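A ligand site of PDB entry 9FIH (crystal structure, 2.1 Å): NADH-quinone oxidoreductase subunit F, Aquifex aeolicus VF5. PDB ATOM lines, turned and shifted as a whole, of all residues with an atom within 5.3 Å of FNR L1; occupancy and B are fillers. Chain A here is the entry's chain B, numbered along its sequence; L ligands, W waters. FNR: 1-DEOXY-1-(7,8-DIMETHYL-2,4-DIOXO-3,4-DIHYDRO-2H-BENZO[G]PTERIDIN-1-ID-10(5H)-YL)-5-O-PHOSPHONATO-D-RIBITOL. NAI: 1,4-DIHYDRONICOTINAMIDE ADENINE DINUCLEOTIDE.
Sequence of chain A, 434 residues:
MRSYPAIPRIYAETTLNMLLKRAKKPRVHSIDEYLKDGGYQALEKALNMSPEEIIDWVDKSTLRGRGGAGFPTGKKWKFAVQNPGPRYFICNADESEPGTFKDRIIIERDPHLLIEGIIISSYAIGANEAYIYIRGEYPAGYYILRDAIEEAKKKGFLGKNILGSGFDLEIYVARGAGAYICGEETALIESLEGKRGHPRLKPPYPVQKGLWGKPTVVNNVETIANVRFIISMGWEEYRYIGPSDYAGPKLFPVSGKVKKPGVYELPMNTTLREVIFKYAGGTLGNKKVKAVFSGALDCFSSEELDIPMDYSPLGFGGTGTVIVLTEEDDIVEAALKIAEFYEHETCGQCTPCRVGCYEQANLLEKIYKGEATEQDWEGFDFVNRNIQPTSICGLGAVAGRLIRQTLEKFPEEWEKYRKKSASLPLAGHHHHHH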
ATOM      1  N   GLY A  65      19.035   2.091  29.504  1.00  0.00           N
ATOM      2  CA  GLY A  65      19.391   3.423  29.072  1.00  0.00           C
ATOM      3  C   GLY A  65      20.497   4.027  29.925  1.00  0.00           C
ATOM      4  O   GLY A  65      20.357   4.152  31.148  1.00  0.00           O
ATOM      5  N   ARG A  66      21.596   4.419  29.268  1.00  0.00           N
ATOM      6  CA  ARG A  66      22.790   4.894  29.953  1.00  0.00           C
ATOM      7  C   ARG A  66      22.730   6.407  30.125  1.00  0.00           C
ATOM      8  O   ARG A  66      23.664   7.029  30.632  1.00  0.00           O
ATOM      9  CB  ARG A  66      24.022   4.506  29.130  1.00  0.00           C
ATOM     10  CG  ARG A  66      24.239   3.003  28.944  1.00  0.00           C
ATOM     11  CD  ARG A  66      24.443   2.242  30.239  1.00  0.00           C
ATOM     12  NE  ARG A  66      24.990   0.901  29.978  1.00  0.00           N
ATOM     13  CZ  ARG A  66      24.496  -0.285  30.335  1.00  0.00           C
ATOM     14  NH1 ARG A  66      25.285  -1.350  30.221  1.00  0.00           N
ATOM     15  NH2 ARG A  66      23.273  -0.443  30.822  1.00  0.00           N
ATOM     16  N   GLY A  67      21.606   6.994  29.693  1.00  0.00           N
ATOM     17  CA  GLY A  67      21.385   8.426  29.824  1.00  0.00           C
ATOM     18  C   GLY A  67      21.134   8.798  31.278  1.00  0.00           C
ATOM     19  O   GLY A  67      21.178   9.972  31.622  1.00  0.00           O
ATOM     20  N   GLY A  68      20.837   7.802  32.124  1.00  0.00           N
ATOM     21  CA  GLY A  68      20.659   8.047  33.545  1.00  0.00           C
ATOM     22  C   GLY A  68      19.386   7.429  34.106  1.00  0.00           C
ATOM     23  O   GLY A  68      19.355   7.131  35.292  1.00  0.00           O
ATOM     24  N   ALA A  69      18.331   7.238  33.291  1.00  0.00           N
ATOM     25  CA  ALA A  69      17.084   6.687  33.816  1.00  0.00           C
ATOM     26  C   ALA A  69      17.058   5.154  33.786  1.00  0.00           C
ATOM     27  O   ALA A  69      16.267   4.535  34.491  1.00  0.00           O
ATOM     28  CB  ALA A  69      15.893   7.252  33.087  1.00  0.00           C
ATOM     29  N   GLY A  70      17.893   4.544  32.950  1.00  0.00           N
ATOM     30  CA  GLY A  70      17.991   3.095  32.911  1.00  0.00           C
ATOM     31  C   GLY A  70      16.747   2.398  32.368  1.00  0.00           C
ATOM     32  O   GLY A  70      16.452   1.280  32.779  1.00  0.00           O
ATOM     33  N   PHE A  71      16.035   3.015  31.434  1.00  0.00           N
ATOM     34  CA  PHE A  71      14.883   2.345  30.830  1.00  0.00           C
ATOM     35  C   PHE A  71      15.347   1.232  29.870  1.00  0.00           C
ATOM     36  O   PHE A  71      16.256   1.468  29.074  1.00  0.00           O
ATOM     37  CB  PHE A  71      14.023   3.355  30.080  1.00  0.00           C
ATOM     38  CG  PHE A  71      12.688   2.750  29.705  1.00  0.00           C
ATOM     39  CD1 PHE A  71      11.603   2.803  30.580  1.00  0.00           C
ATOM     40  CD2 PHE A  71      12.525   2.069  28.497  1.00  0.00           C
ATOM     41  CE1 PHE A  71      10.387   2.227  30.250  1.00  0.00           C
ATOM     42  CE2 PHE A  71      11.306   1.506  28.166  1.00  0.00           C
ATOM     43  CZ  PHE A  71      10.241   1.579  29.047  1.00  0.00           C
ATOM     44  N   THR A  73      16.249  -0.787  26.776  1.00  0.00           N
ATOM     45  CA  THR A  73      16.400  -0.261  25.436  1.00  0.00           C
ATOM     46  C   THR A  73      15.546  -1.051  24.448  1.00  0.00           C
ATOM     47  O   THR A  73      14.896  -0.471  23.591  1.00  0.00           O
ATOM     48  CB  THR A  73      17.866  -0.274  25.055  1.00  0.00           C
ATOM     49  OG1 THR A  73      18.571   0.361  26.124  1.00  0.00           O
ATOM     50  CG2 THR A  73      18.123   0.428  23.733  1.00  0.00           C
ATOM     51  N   LYS A  76      11.919  -0.202  24.637  1.00  0.00           N
ATOM     52  CA  LYS A  76      11.685   1.114  24.042  1.00  0.00           C
ATOM     53  C   LYS A  76      11.514   0.975  22.531  1.00  0.00           C
ATOM     54  O   LYS A  76      10.603   1.570  21.945  1.00  0.00           O
ATOM     55  CB  LYS A  76      12.809   2.107  24.373  1.00  0.00           C
ATOM     56  CG  LYS A  76      12.546   3.526  23.936  1.00  0.00           C
ATOM     57  CD  LYS A  76      13.695   4.501  24.177  1.00  0.00           C
ATOM     58  CE  LYS A  76      14.173   4.601  25.604  1.00  0.00           C
ATOM     59  NZ  LYS A  76      15.129   5.698  25.729  1.00  0.00           N
ATOM     60  N   ASN A  92      21.250  11.082  21.643  1.00  0.00           N
ATOM     61  CA  ASN A  92      21.291  12.177  22.598  1.00  0.00           C
ATOM     62  C   ASN A  92      22.732  12.370  23.050  1.00  0.00           C
ATOM     63  O   ASN A  92      23.212  11.608  23.885  1.00  0.00           O
ATOM     64  CB  ASN A  92      20.356  11.915  23.782  1.00  0.00           C
ATOM     65  CG  ASN A  92      20.176  13.130  24.653  1.00  0.00           C
ATOM     66  OD1 ASN A  92      20.963  14.081  24.608  1.00  0.00           O
ATOM     67  ND2 ASN A  92      19.127  13.083  25.464  1.00  0.00           N
ATOM     68  N   ALA A  93      23.391  13.422  22.520  1.00  0.00           N
ATOM     69  CA  ALA A  93      24.734  13.790  22.899  1.00  0.00           C
ATOM     70  C   ALA A  93      24.742  15.177  23.566  1.00  0.00           C
ATOM     71  O   ALA A  93      25.701  15.944  23.420  1.00  0.00           O
ATOM     72  CB  ALA A  93      25.619  13.720  21.682  1.00  0.00           C
ATOM     73  N   ASP A  94      23.706  15.471  24.348  1.00  0.00           N
ATOM     74  CA  ASP A  94      23.635  16.782  24.991  1.00  0.00           C
ATOM     75  C   ASP A  94      24.500  16.838  26.252  1.00  0.00           C
ATOM     76  O   ASP A  94      24.850  17.937  26.659  1.00  0.00           O
ATOM     77  CB  ASP A  94      22.213  17.224  25.285  1.00  0.00           C
ATOM     78  CG  ASP A  94      22.083  18.709  25.538  1.00  0.00           C
ATOM     79  OD1 ASP A  94      22.365  19.482  24.595  1.00  0.00           O
ATOM     80  OD2 ASP A  94      21.753  19.084  26.685  1.00  0.00           O
ATOM     81  N   GLU A  95      24.851  15.668  26.828  1.00  0.00           N
ATOM     82  CA  GLU A  95      25.590  15.507  28.070  1.00  0.00           C
ATOM     83  C   GLU A  95      25.966  16.827  28.742  1.00  0.00           C
ATOM     84  O   GLU A  95      27.014  17.394  28.442  1.00  0.00           O
ATOM     85  CB  GLU A  95      26.855  14.685  27.782  1.00  0.00           C
ATOM     86  CG  GLU A  95      27.757  14.439  28.990  1.00  0.00           C
ATOM     87  CD  GLU A  95      28.865  13.413  28.739  1.00  0.00           C
ATOM     88  OE1 GLU A  95      29.842  13.727  28.001  1.00  0.00           O
ATOM     89  OE2 GLU A  95      28.714  12.304  29.308  1.00  0.00           O
ATOM     90  N   SER A  96      25.138  17.276  29.700  1.00  0.00           N
ATOM     91  CA  SER A  96      25.376  18.527  30.413  1.00  0.00           C
ATOM     92  C   SER A  96      25.181  18.437  31.928  1.00  0.00           C
ATOM     93  O   SER A  96      25.241  19.458  32.599  1.00  0.00           O
ATOM     94  CB  SER A  96      24.479  19.600  29.874  1.00  0.00           C
ATOM     95  OG  SER A  96      24.854  19.988  28.570  1.00  0.00           O
ATOM     96  N   ASP A 103      30.268  10.547  27.740  1.00  0.00           N
ATOM     97  CA  ASP A 103      29.854  10.378  26.360  1.00  0.00           C
ATOM     98  C   ASP A 103      30.855  11.034  25.420  1.00  0.00           C
ATOM     99  O   ASP A 103      31.116  10.490  24.339  1.00  0.00           O
ATOM    100  CB  ASP A 103      28.463  10.939  26.088  1.00  0.00           C
ATOM    101  CG  ASP A 103      27.330  10.329  26.885  1.00  0.00           C
ATOM    102  OD1 ASP A 103      27.513   9.232  27.451  1.00  0.00           O
ATOM    103  OD2 ASP A 103      26.256  10.996  26.949  1.00  0.00           O
ATOM    104  N   TYR A 180      20.854  23.132  29.214  1.00  0.00           N
ATOM    105  CA  TYR A 180      20.851  21.794  29.796  1.00  0.00           C
ATOM    106  C   TYR A 180      19.542  21.072  29.506  1.00  0.00           C
ATOM    107  O   TYR A 180      19.535  19.856  29.334  1.00  0.00           O
ATOM    108  CB  TYR A 180      21.075  21.986  31.294  1.00  0.00           C
ATOM    109  CG  TYR A 180      20.735  20.838  32.233  1.00  0.00           C
ATOM    110  CD1 TYR A 180      21.583  19.753  32.384  1.00  0.00           C
ATOM    111  CD2 TYR A 180      19.589  20.862  33.009  1.00  0.00           C
ATOM    112  CE1 TYR A 180      21.275  18.728  33.257  1.00  0.00           C
ATOM    113  CE2 TYR A 180      19.280  19.845  33.894  1.00  0.00           C
ATOM    114  CZ  TYR A 180      20.132  18.768  34.040  1.00  0.00           C
ATOM    115  OH  TYR A 180      19.861  17.766  34.919  1.00  0.00           O
ATOM    116  N   ILE A 181      18.430  21.824  29.488  1.00  0.00           N
ATOM    117  CA  ILE A 181      17.099  21.256  29.339  1.00  0.00           C
ATOM    118  C   ILE A 181      16.952  20.591  27.965  1.00  0.00           C
ATOM    119  O   ILE A 181      16.106  19.703  27.812  1.00  0.00           O
ATOM    120  CB  ILE A 181      16.015  22.333  29.548  1.00  0.00           C
ATOM    121  CG1 ILE A 181      14.656  21.740  29.725  1.00  0.00           C
ATOM    122  CG2 ILE A 181      16.000  23.375  28.424  1.00  0.00           C
ATOM    123  CD1 ILE A 181      14.551  20.738  30.850  1.00  0.00           C
ATOM    124  N   GLY A 183      18.664  18.458  26.740  1.00  0.00           N
ATOM    125  CA  GLY A 183      19.000  17.045  26.861  1.00  0.00           C
ATOM    126  C   GLY A 183      17.808  16.191  27.284  1.00  0.00           C
ATOM    127  O   GLY A 183      17.832  14.969  27.129  1.00  0.00           O
ATOM    128  N   GLU A 184      16.779  16.852  27.870  1.00  0.00           N
ATOM    129  CA  GLU A 184      15.501  16.187  28.107  1.00  0.00           C
ATOM    130  C   GLU A 184      14.919  15.859  26.723  1.00  0.00           C
ATOM    131  O   GLU A 184      14.840  16.730  25.851  1.00  0.00           O
ATOM    132  CB  GLU A 184      14.614  17.079  28.972  1.00  0.00           C
ATOM    133  CG  GLU A 184      13.457  16.342  29.630  1.00  0.00           C
ATOM    134  CD  GLU A 184      12.234  16.125  28.753  1.00  0.00           C
ATOM    135  OE1 GLU A 184      12.163  16.702  27.671  1.00  0.00           O
ATOM    136  OE2 GLU A 184      11.349  15.357  29.186  1.00  0.00           O
ATOM    137  N   GLU A 185      14.547  14.579  26.527  1.00  0.00           N
ATOM    138  CA  GLU A 185      14.304  14.071  25.171  1.00  0.00           C
ATOM    139  C   GLU A 185      13.243  14.885  24.413  1.00  0.00           C
ATOM    140  O   GLU A 185      13.347  15.052  23.206  1.00  0.00           O
ATOM    141  CB  GLU A 185      13.950  12.595  25.236  1.00  0.00           C
ATOM    142  CG  GLU A 185      12.709  12.285  26.062  1.00  0.00           C
ATOM    143  CD  GLU A 185      12.305  10.818  26.098  1.00  0.00           C
ATOM    144  OE1 GLU A 185      13.005  10.003  25.459  1.00  0.00           O
ATOM    145  OE2 GLU A 185      11.297  10.505  26.770  1.00  0.00           O
ATOM    146  N   VAL A 218      14.674   8.060  21.197  1.00  0.00           N
ATOM    147  CA  VAL A 218      15.803   8.822  21.681  1.00  0.00           C
ATOM    148  C   VAL A 218      16.627   7.889  22.563  1.00  0.00           C
ATOM    149  O   VAL A 218      16.120   7.326  23.541  1.00  0.00           O
ATOM    150  CB  VAL A 218      15.407  10.097  22.441  1.00  0.00           C
ATOM    151  CG1 VAL A 218      16.617  10.915  22.878  1.00  0.00           C
ATOM    152  CG2 VAL A 218      14.459  10.983  21.646  1.00  0.00           C
ATOM    153  N   ASN A 219      17.916   7.742  22.229  1.00  0.00           N
ATOM    154  CA  ASN A 219      18.845   7.011  23.087  1.00  0.00           C
ATOM    155  C   ASN A 219      20.109   7.828  23.323  1.00  0.00           C
ATOM    156  O   ASN A 219      20.504   8.635  22.491  1.00  0.00           O
ATOM    157  CB  ASN A 219      19.189   5.643  22.526  1.00  0.00           C
ATOM    158  CG  ASN A 219      18.224   4.577  22.977  1.00  0.00           C
ATOM    159  OD1 ASN A 219      17.978   4.410  24.184  1.00  0.00           O
ATOM    160  ND2 ASN A 219      17.666   3.846  22.026  1.00  0.00           N
ATOM    161  N   ASN A 220      20.722   7.583  24.488  1.00  0.00           N
ATOM    162  CA  ASN A 220      21.968   8.195  24.900  1.00  0.00           C
ATOM    163  C   ASN A 220      23.162   7.601  24.131  1.00  0.00           C
ATOM    164  O   ASN A 220      23.122   6.432  23.757  1.00  0.00           O
ATOM    165  CB  ASN A 220      22.099   8.072  26.417  1.00  0.00           C
ATOM    166  CG  ASN A 220      23.429   8.551  26.915  1.00  0.00           C
ATOM    167  OD1 ASN A 220      23.680   9.772  26.999  1.00  0.00           O
ATOM    168  ND2 ASN A 220      24.294   7.604  27.257  1.00  0.00           N
ATOM    169  N   VAL A 221      24.201   8.422  23.912  1.00  0.00           N
ATOM    170  CA  VAL A 221      25.441   8.044  23.257  1.00  0.00           C
ATOM    171  C   VAL A 221      25.951   6.699  23.775  1.00  0.00           C
ATOM    172  O   VAL A 221      26.249   5.815  22.990  1.00  0.00           O
ATOM    173  CB  VAL A 221      26.510   9.148  23.425  1.00  0.00           C
ATOM    174  CG1 VAL A 221      27.930   8.682  23.113  1.00  0.00           C
ATOM    175  CG2 VAL A 221      26.187  10.368  22.565  1.00  0.00           C
ATOM    176  N   THR A 223      24.465   4.302  25.541  1.00  0.00           N
ATOM    177  CA  THR A 223      23.545   3.228  25.197  1.00  0.00           C
ATOM    178  C   THR A 223      23.865   2.703  23.807  1.00  0.00           C
ATOM    179  O   THR A 223      24.030   1.506  23.607  1.00  0.00           O
ATOM    180  CB  THR A 223      22.099   3.699  25.250  1.00  0.00           C
ATOM    181  OG1 THR A 223      21.923   4.420  26.477  1.00  0.00           O
ATOM    182  CG2 THR A 223      21.131   2.539  25.099  1.00  0.00           C
ATOM    183  N   CYS A 393       8.530  17.746  33.572  1.00  0.00           N
ATOM    184  CA  CYS A 393       9.771  17.059  33.230  1.00  0.00           C
ATOM    185  C   CYS A 393      10.599  16.839  34.497  1.00  0.00           C
ATOM    186  O   CYS A 393      10.254  17.336  35.575  1.00  0.00           O
ATOM    187  CB  CYS A 393      10.555  17.778  32.141  1.00  0.00           C
ATOM    188  SG  CYS A 393      11.848  18.902  32.720  1.00  0.00           S
ATOM    189  N   GLY A 394      11.698  16.096  34.334  1.00  0.00           N
ATOM    190  CA  GLY A 394      12.467  15.543  35.437  1.00  0.00           C
ATOM    191  C   GLY A 394      13.274  16.610  36.164  1.00  0.00           C
ATOM    192  O   GLY A 394      13.692  16.386  37.300  1.00  0.00           O
ATOM    193  N   LEU A 395      13.526  17.762  35.525  1.00  0.00           N
ATOM    194  CA  LEU A 395      14.286  18.818  36.175  1.00  0.00           C
ATOM    195  C   LEU A 395      13.519  19.292  37.409  1.00  0.00           C
ATOM    196  O   LEU A 395      14.061  19.324  38.519  1.00  0.00           O
ATOM    197  CB  LEU A 395      14.534  19.950  35.193  1.00  0.00           C
ATOM    198  CG  LEU A 395      15.572  21.000  35.621  1.00  0.00           C
ATOM    199  CD1 LEU A 395      16.192  21.674  34.423  1.00  0.00           C
ATOM    200  CD2 LEU A 395      14.996  22.051  36.551  1.00  0.00           C
HETATM  201  C9A FNR L   1      17.831  14.234  30.483  1.00  0.00           C
HETATM  202  N10 FNR L   1      18.284  13.065  29.795  1.00  0.00           N
HETATM  203  CAA FNR L   1      19.483  13.110  29.089  1.00  0.00           C
HETATM  204  N1  FNR L   1      19.893  11.983  28.410  1.00  0.00           N
HETATM  205  C2  FNR L   1      21.033  11.959  27.650  1.00  0.00           C
HETATM  206  O2  FNR L   1      21.315  11.020  26.928  1.00  0.00           O
HETATM  207  N3  FNR L   1      21.816  13.085  27.691  1.00  0.00           N
HETATM  208  C4  FNR L   1      21.505  14.271  28.323  1.00  0.00           C
HETATM  209  O4  FNR L   1      22.275  15.214  28.230  1.00  0.00           O
HETATM  210  C4A FNR L   1      20.251  14.238  29.040  1.00  0.00           C
HETATM  211  N5  FNR L   1      19.811  15.368  29.678  1.00  0.00           N
HETATM  212  C5A FNR L   1      18.616  15.390  30.389  1.00  0.00           C
HETATM  213  C6  FNR L   1      18.192  16.554  31.032  1.00  0.00           C
HETATM  214  C7  FNR L   1      17.033  16.580  31.779  1.00  0.00           C
HETATM  215  C7M FNR L   1      16.597  17.860  32.452  1.00  0.00           C
HETATM  216  C8  FNR L   1      16.255  15.420  31.894  1.00  0.00           C
HETATM  217  C8M FNR L   1      15.062  15.404  32.814  1.00  0.00           C
HETATM  218  C9  FNR L   1      16.654  14.264  31.242  1.00  0.00           C
HETATM  219  C1' FNR L   1      17.478  11.829  29.785  1.00  0.00           C
HETATM  220  C2' FNR L   1      16.626  11.825  28.515  1.00  0.00           C
HETATM  221  O2' FNR L   1      15.407  12.555  28.718  1.00  0.00           O
HETATM  222  C3' FNR L   1      16.312  10.377  28.105  1.00  0.00           C
HETATM  223  O3' FNR L   1      15.932   9.656  29.270  1.00  0.00           O
HETATM  224  C4' FNR L   1      17.465   9.625  27.442  1.00  0.00           C
HETATM  225  O4' FNR L   1      18.146  10.397  26.451  1.00  0.00           O
HETATM  226  C5' FNR L   1      16.967   8.332  26.850  1.00  0.00           C
HETATM  227  O5' FNR L   1      18.076   7.531  26.380  1.00  0.00           O
HETATM  228  P   FNR L   1      18.505   6.181  27.170  1.00  0.00           P
HETATM  229  O1P FNR L   1      19.522   5.561  26.207  1.00  0.00           O
HETATM  230  O2P FNR L   1      17.270   5.329  27.335  1.00  0.00           O
HETATM  231  O3P FNR L   1      19.142   6.579  28.485  1.00  0.00           O
HETATM  232  PA  NAI L   2      12.226   8.606  32.353  1.00  0.00           P
HETATM  233  O1A NAI L   2      12.427   7.627  33.428  1.00  0.00           O
HETATM  234  O2A NAI L   2      10.985   9.366  32.401  1.00  0.00           O
HETATM  235  O5B NAI L   2      12.255   7.961  30.874  1.00  0.00           O
HETATM  236  C5B NAI L   2      13.426   7.206  30.448  1.00  0.00           C
HETATM  237  C4B NAI L   2      13.325   6.828  29.009  1.00  0.00           C
HETATM  238  O4B NAI L   2      12.350   5.765  28.902  1.00  0.00           O
HETATM  239  C3B NAI L   2      12.848   7.930  28.076  1.00  0.00           C
HETATM  240  O3B NAI L   2      13.416   7.785  26.778  1.00  0.00           O
HETATM  241  C2B NAI L   2      11.337   7.703  28.021  1.00  0.00           C
HETATM  242  O2B NAI L   2      10.791   8.130  26.789  1.00  0.00           O
HETATM  243  C1B NAI L   2      11.277   6.173  28.090  1.00  0.00           C
HETATM  244  N9A NAI L   2      10.062   5.650  28.686  1.00  0.00           N
HETATM  245  C8A NAI L   2       9.733   5.644  30.013  1.00  0.00           C
HETATM  246  N7A NAI L   2       8.578   5.102  30.283  1.00  0.00           N
HETATM  247  C5A NAI L   2       8.101   4.715  29.040  1.00  0.00           C
HETATM  248  C6A NAI L   2       6.911   4.088  28.653  1.00  0.00           C
HETATM  249  N6A NAI L   2       5.959   3.724  29.499  1.00  0.00           N
HETATM  250  N1A NAI L   2       6.739   3.837  27.333  1.00  0.00           N
HETATM  251  C2A NAI L   2       7.702   4.203  26.479  1.00  0.00           C
HETATM  252  N3A NAI L   2       8.863   4.811  26.728  1.00  0.00           N
HETATM  253  C4A NAI L   2       9.008   5.048  28.046  1.00  0.00           C
HETATM  254  O3  NAI L   2      13.426   9.638  32.483  1.00  0.00           O
HETATM  255  PN  NAI L   2      13.844  11.011  31.820  1.00  0.00           P
HETATM  256  O1N NAI L   2      12.910  12.044  32.434  1.00  0.00           O
HETATM  257  O2N NAI L   2      13.800  11.031  30.317  1.00  0.00           O
HETATM  258  O5D NAI L   2      15.336  11.249  32.325  1.00  0.00           O
HETATM  259  C5D NAI L   2      15.733  11.444  33.710  1.00  0.00           C
HETATM  260  C4D NAI L   2      17.206  11.126  33.839  1.00  0.00           C
HETATM  261  O4D NAI L   2      17.981  12.071  33.077  1.00  0.00           O
HETATM  262  C3D NAI L   2      17.778  11.224  35.262  1.00  0.00           C
HETATM  263  O3D NAI L   2      17.839   9.946  35.871  1.00  0.00           O
HETATM  264  C2D NAI L   2      19.211  11.764  35.044  1.00  0.00           C
HETATM  265  O2D NAI L   2      20.187  10.836  35.490  1.00  0.00           O
HETATM  266  C1D NAI L   2      19.310  11.892  33.525  1.00  0.00           C
HETATM  267  N1N NAI L   2      20.105  13.038  33.076  1.00  0.00           N
HETATM  268  C2N NAI L   2      21.256  12.878  32.317  1.00  0.00           C
HETATM  269  C3N NAI L   2      22.021  13.922  31.927  1.00  0.00           C
HETATM  270  C7N NAI L   2      23.296  13.671  31.152  1.00  0.00           C
HETATM  271  O7N NAI L   2      24.008  14.640  30.844  1.00  0.00           O
HETATM  272  N7N NAI L   2      23.588  12.414  30.802  1.00  0.00           N
HETATM  273  C4N NAI L   2      21.614  15.335  32.259  1.00  0.00           C
HETATM  274  C5N NAI L   2      20.383  15.373  33.067  1.00  0.00           C
HETATM  275  C6N NAI L   2      19.718  14.297  33.431  1.00  0.00           C
HETATM  276  O   HOH W   1      16.993   2.762  26.674  1.00  0.00           O
HETATM  277  O   HOH W   2      16.446   5.411  30.036  1.00  0.00           O
HETATM  278  O   HOH W   3      21.534  17.884  29.080  1.00  0.00           O
HETATM  279  O   HOH W   4      17.820   7.756  30.531  1.00  0.00           O
HETATM  280  O   HOH W   5      24.338  12.705  26.183  1.00  0.00           O
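O of Gly 183 is in hydrogen-bond range of ND2 of Asn 92 (2.8 Å).
The side-chain amino group (NZ) of Lys 76 sits at hydrogen-bond distance from the side-chain amide oxygen (OD1) of Asn 219.
O of Gly 65 lies within hydrogen-bond range of N of Gly 70 (3.1 Å).
ND2 of Asn 220 lies close to O of Arg 66 (3.5 Å).
NZ of Lys 76 sits at hydrogen-bond distance from O of Val 218 (2.9 Å).
The side-chain amide oxygen (OD1) of Asn 220 lies close to the side-chain carboxylate (OD2) of Asp 103 (2.9 Å).
The backbone NH (N) of Asn 92 is in hydrogen-bond range of the backbone carbonyl oxygen (O) of Asn 219 (2.7 Å).
O of Asp 94 is in hydrogen-bond range of OG of Ser 96 (2.8 Å).
Water W1 lies within hydrogen-bond range of an oxygen (O2P) of FNR L1, the backbone carbonyl oxygen of Phe 71, the side-chain hydroxyl of Thr 73 and the side-chain amide oxygen of Asn 219.
Water W4 lies within hydrogen-bond range of an oxygen (O3P) of FNR L1 (2.7 Å), the backbone NH of Ala 69 (2.9 Å) and the backbone NH of Gly 68 (3.4 Å).
Water W2 lies within hydrogen-bond range of N of Phe 71 (2.8 Å), O2P of FNR L1 (2.8 Å) and N of Gly 70 (3.4 Å).
O5' of FNR L1 lies close to O of Val 218 (3.5 Å).
Gly 65 touches FNR L1 (CA to O3P, 3.2 Å).
C of Asp 94 touches O4 of FNR L1, at 3.4 Å.
Ser 96 touches FNR L1 (N to O4, 3.8 Å).
Tyr 180 touches FNR L1.
Ile 181 touches FNR L1.
Glu 184 touches FNR L1 (N to C5A, 3.4 Å).
CA of Gly 394 touches C8M of FNR L1, at 3.7 Å.
Leu 395 touches FNR L1 (N to C8M, 3.9 Å).
Hydrophobic or aromatic side chains that line FNR L1: Tyr 180, Ile 181 and Val 218.
19 residues have an atom within 4 Å of FNR L1: Gly 65, Arg 66, Gly 67, Lys 76, Asn 92, Asp 94, Glu 95, Ser 96, Tyr 180, Ile 181, Gly 183, Glu 184, Glu 185, Val 218, Asn 219, Asn 220, Thr 223, Gly 394 and Leu 395.
O2N of NAI L2 lies within hydrogen-bond range of O2' of FNR L1 (2.7 Å).
O3D of NAI L2 lies within hydrogen-bond range of O of Gly 68.
NZ of Lys 76 is in salt-bridge range of O2P of FNR L1 (2.7 Å).
The backbone NH (N) of Ser 96 sits at hydrogen-bond distance from an oxygen (O7N) of NAI L2.
O of Gly 183 sits close to N5 of FNR L1 (3.3 Å).
The side-chain hydroxyl (OG1) of Thr 223 lies within hydrogen-bond range of an oxygen (O1P) of FNR L1 (2.7 Å).
OE2 of Glu 185 lies within hydrogen-bond range of O2B of NAI L2 (2.4 Å).
O3B of NAI L2 is in hydrogen-bond range of NZ of Lys 76, 2.9 Å away.
ND2 of Asn 92 lies within hydrogen-bond range of O4' of FNR L1 (3.0 Å).
An oxygen (O3P) of FNR L1 is in hydrogen-bond range of the backbone NH (N) of Gly 67.
The backbone NH of Glu 185 sits at hydrogen-bond distance from an oxygen (O2') of FNR L1 (3.1 Å).
O2 of FNR L1 sits close to OD1 of Asn 220 (2.7 Å).
The side-chain amide oxygen (OD1) of Asn 219 sits close to an oxygen (O1P) of FNR L1, 2.8 Å away.
The backbone NH (N) of Asn 220 lies within hydrogen-bond range of an oxygen (O1P) of FNR L1.
The backbone NH (N) of Glu 95 sits at hydrogen-bond distance from an oxygen (O4) of FNR L1 (3.0 Å).
N of Arg 66 sits at hydrogen-bond distance from O3P of FNR L1 (3.4 Å).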
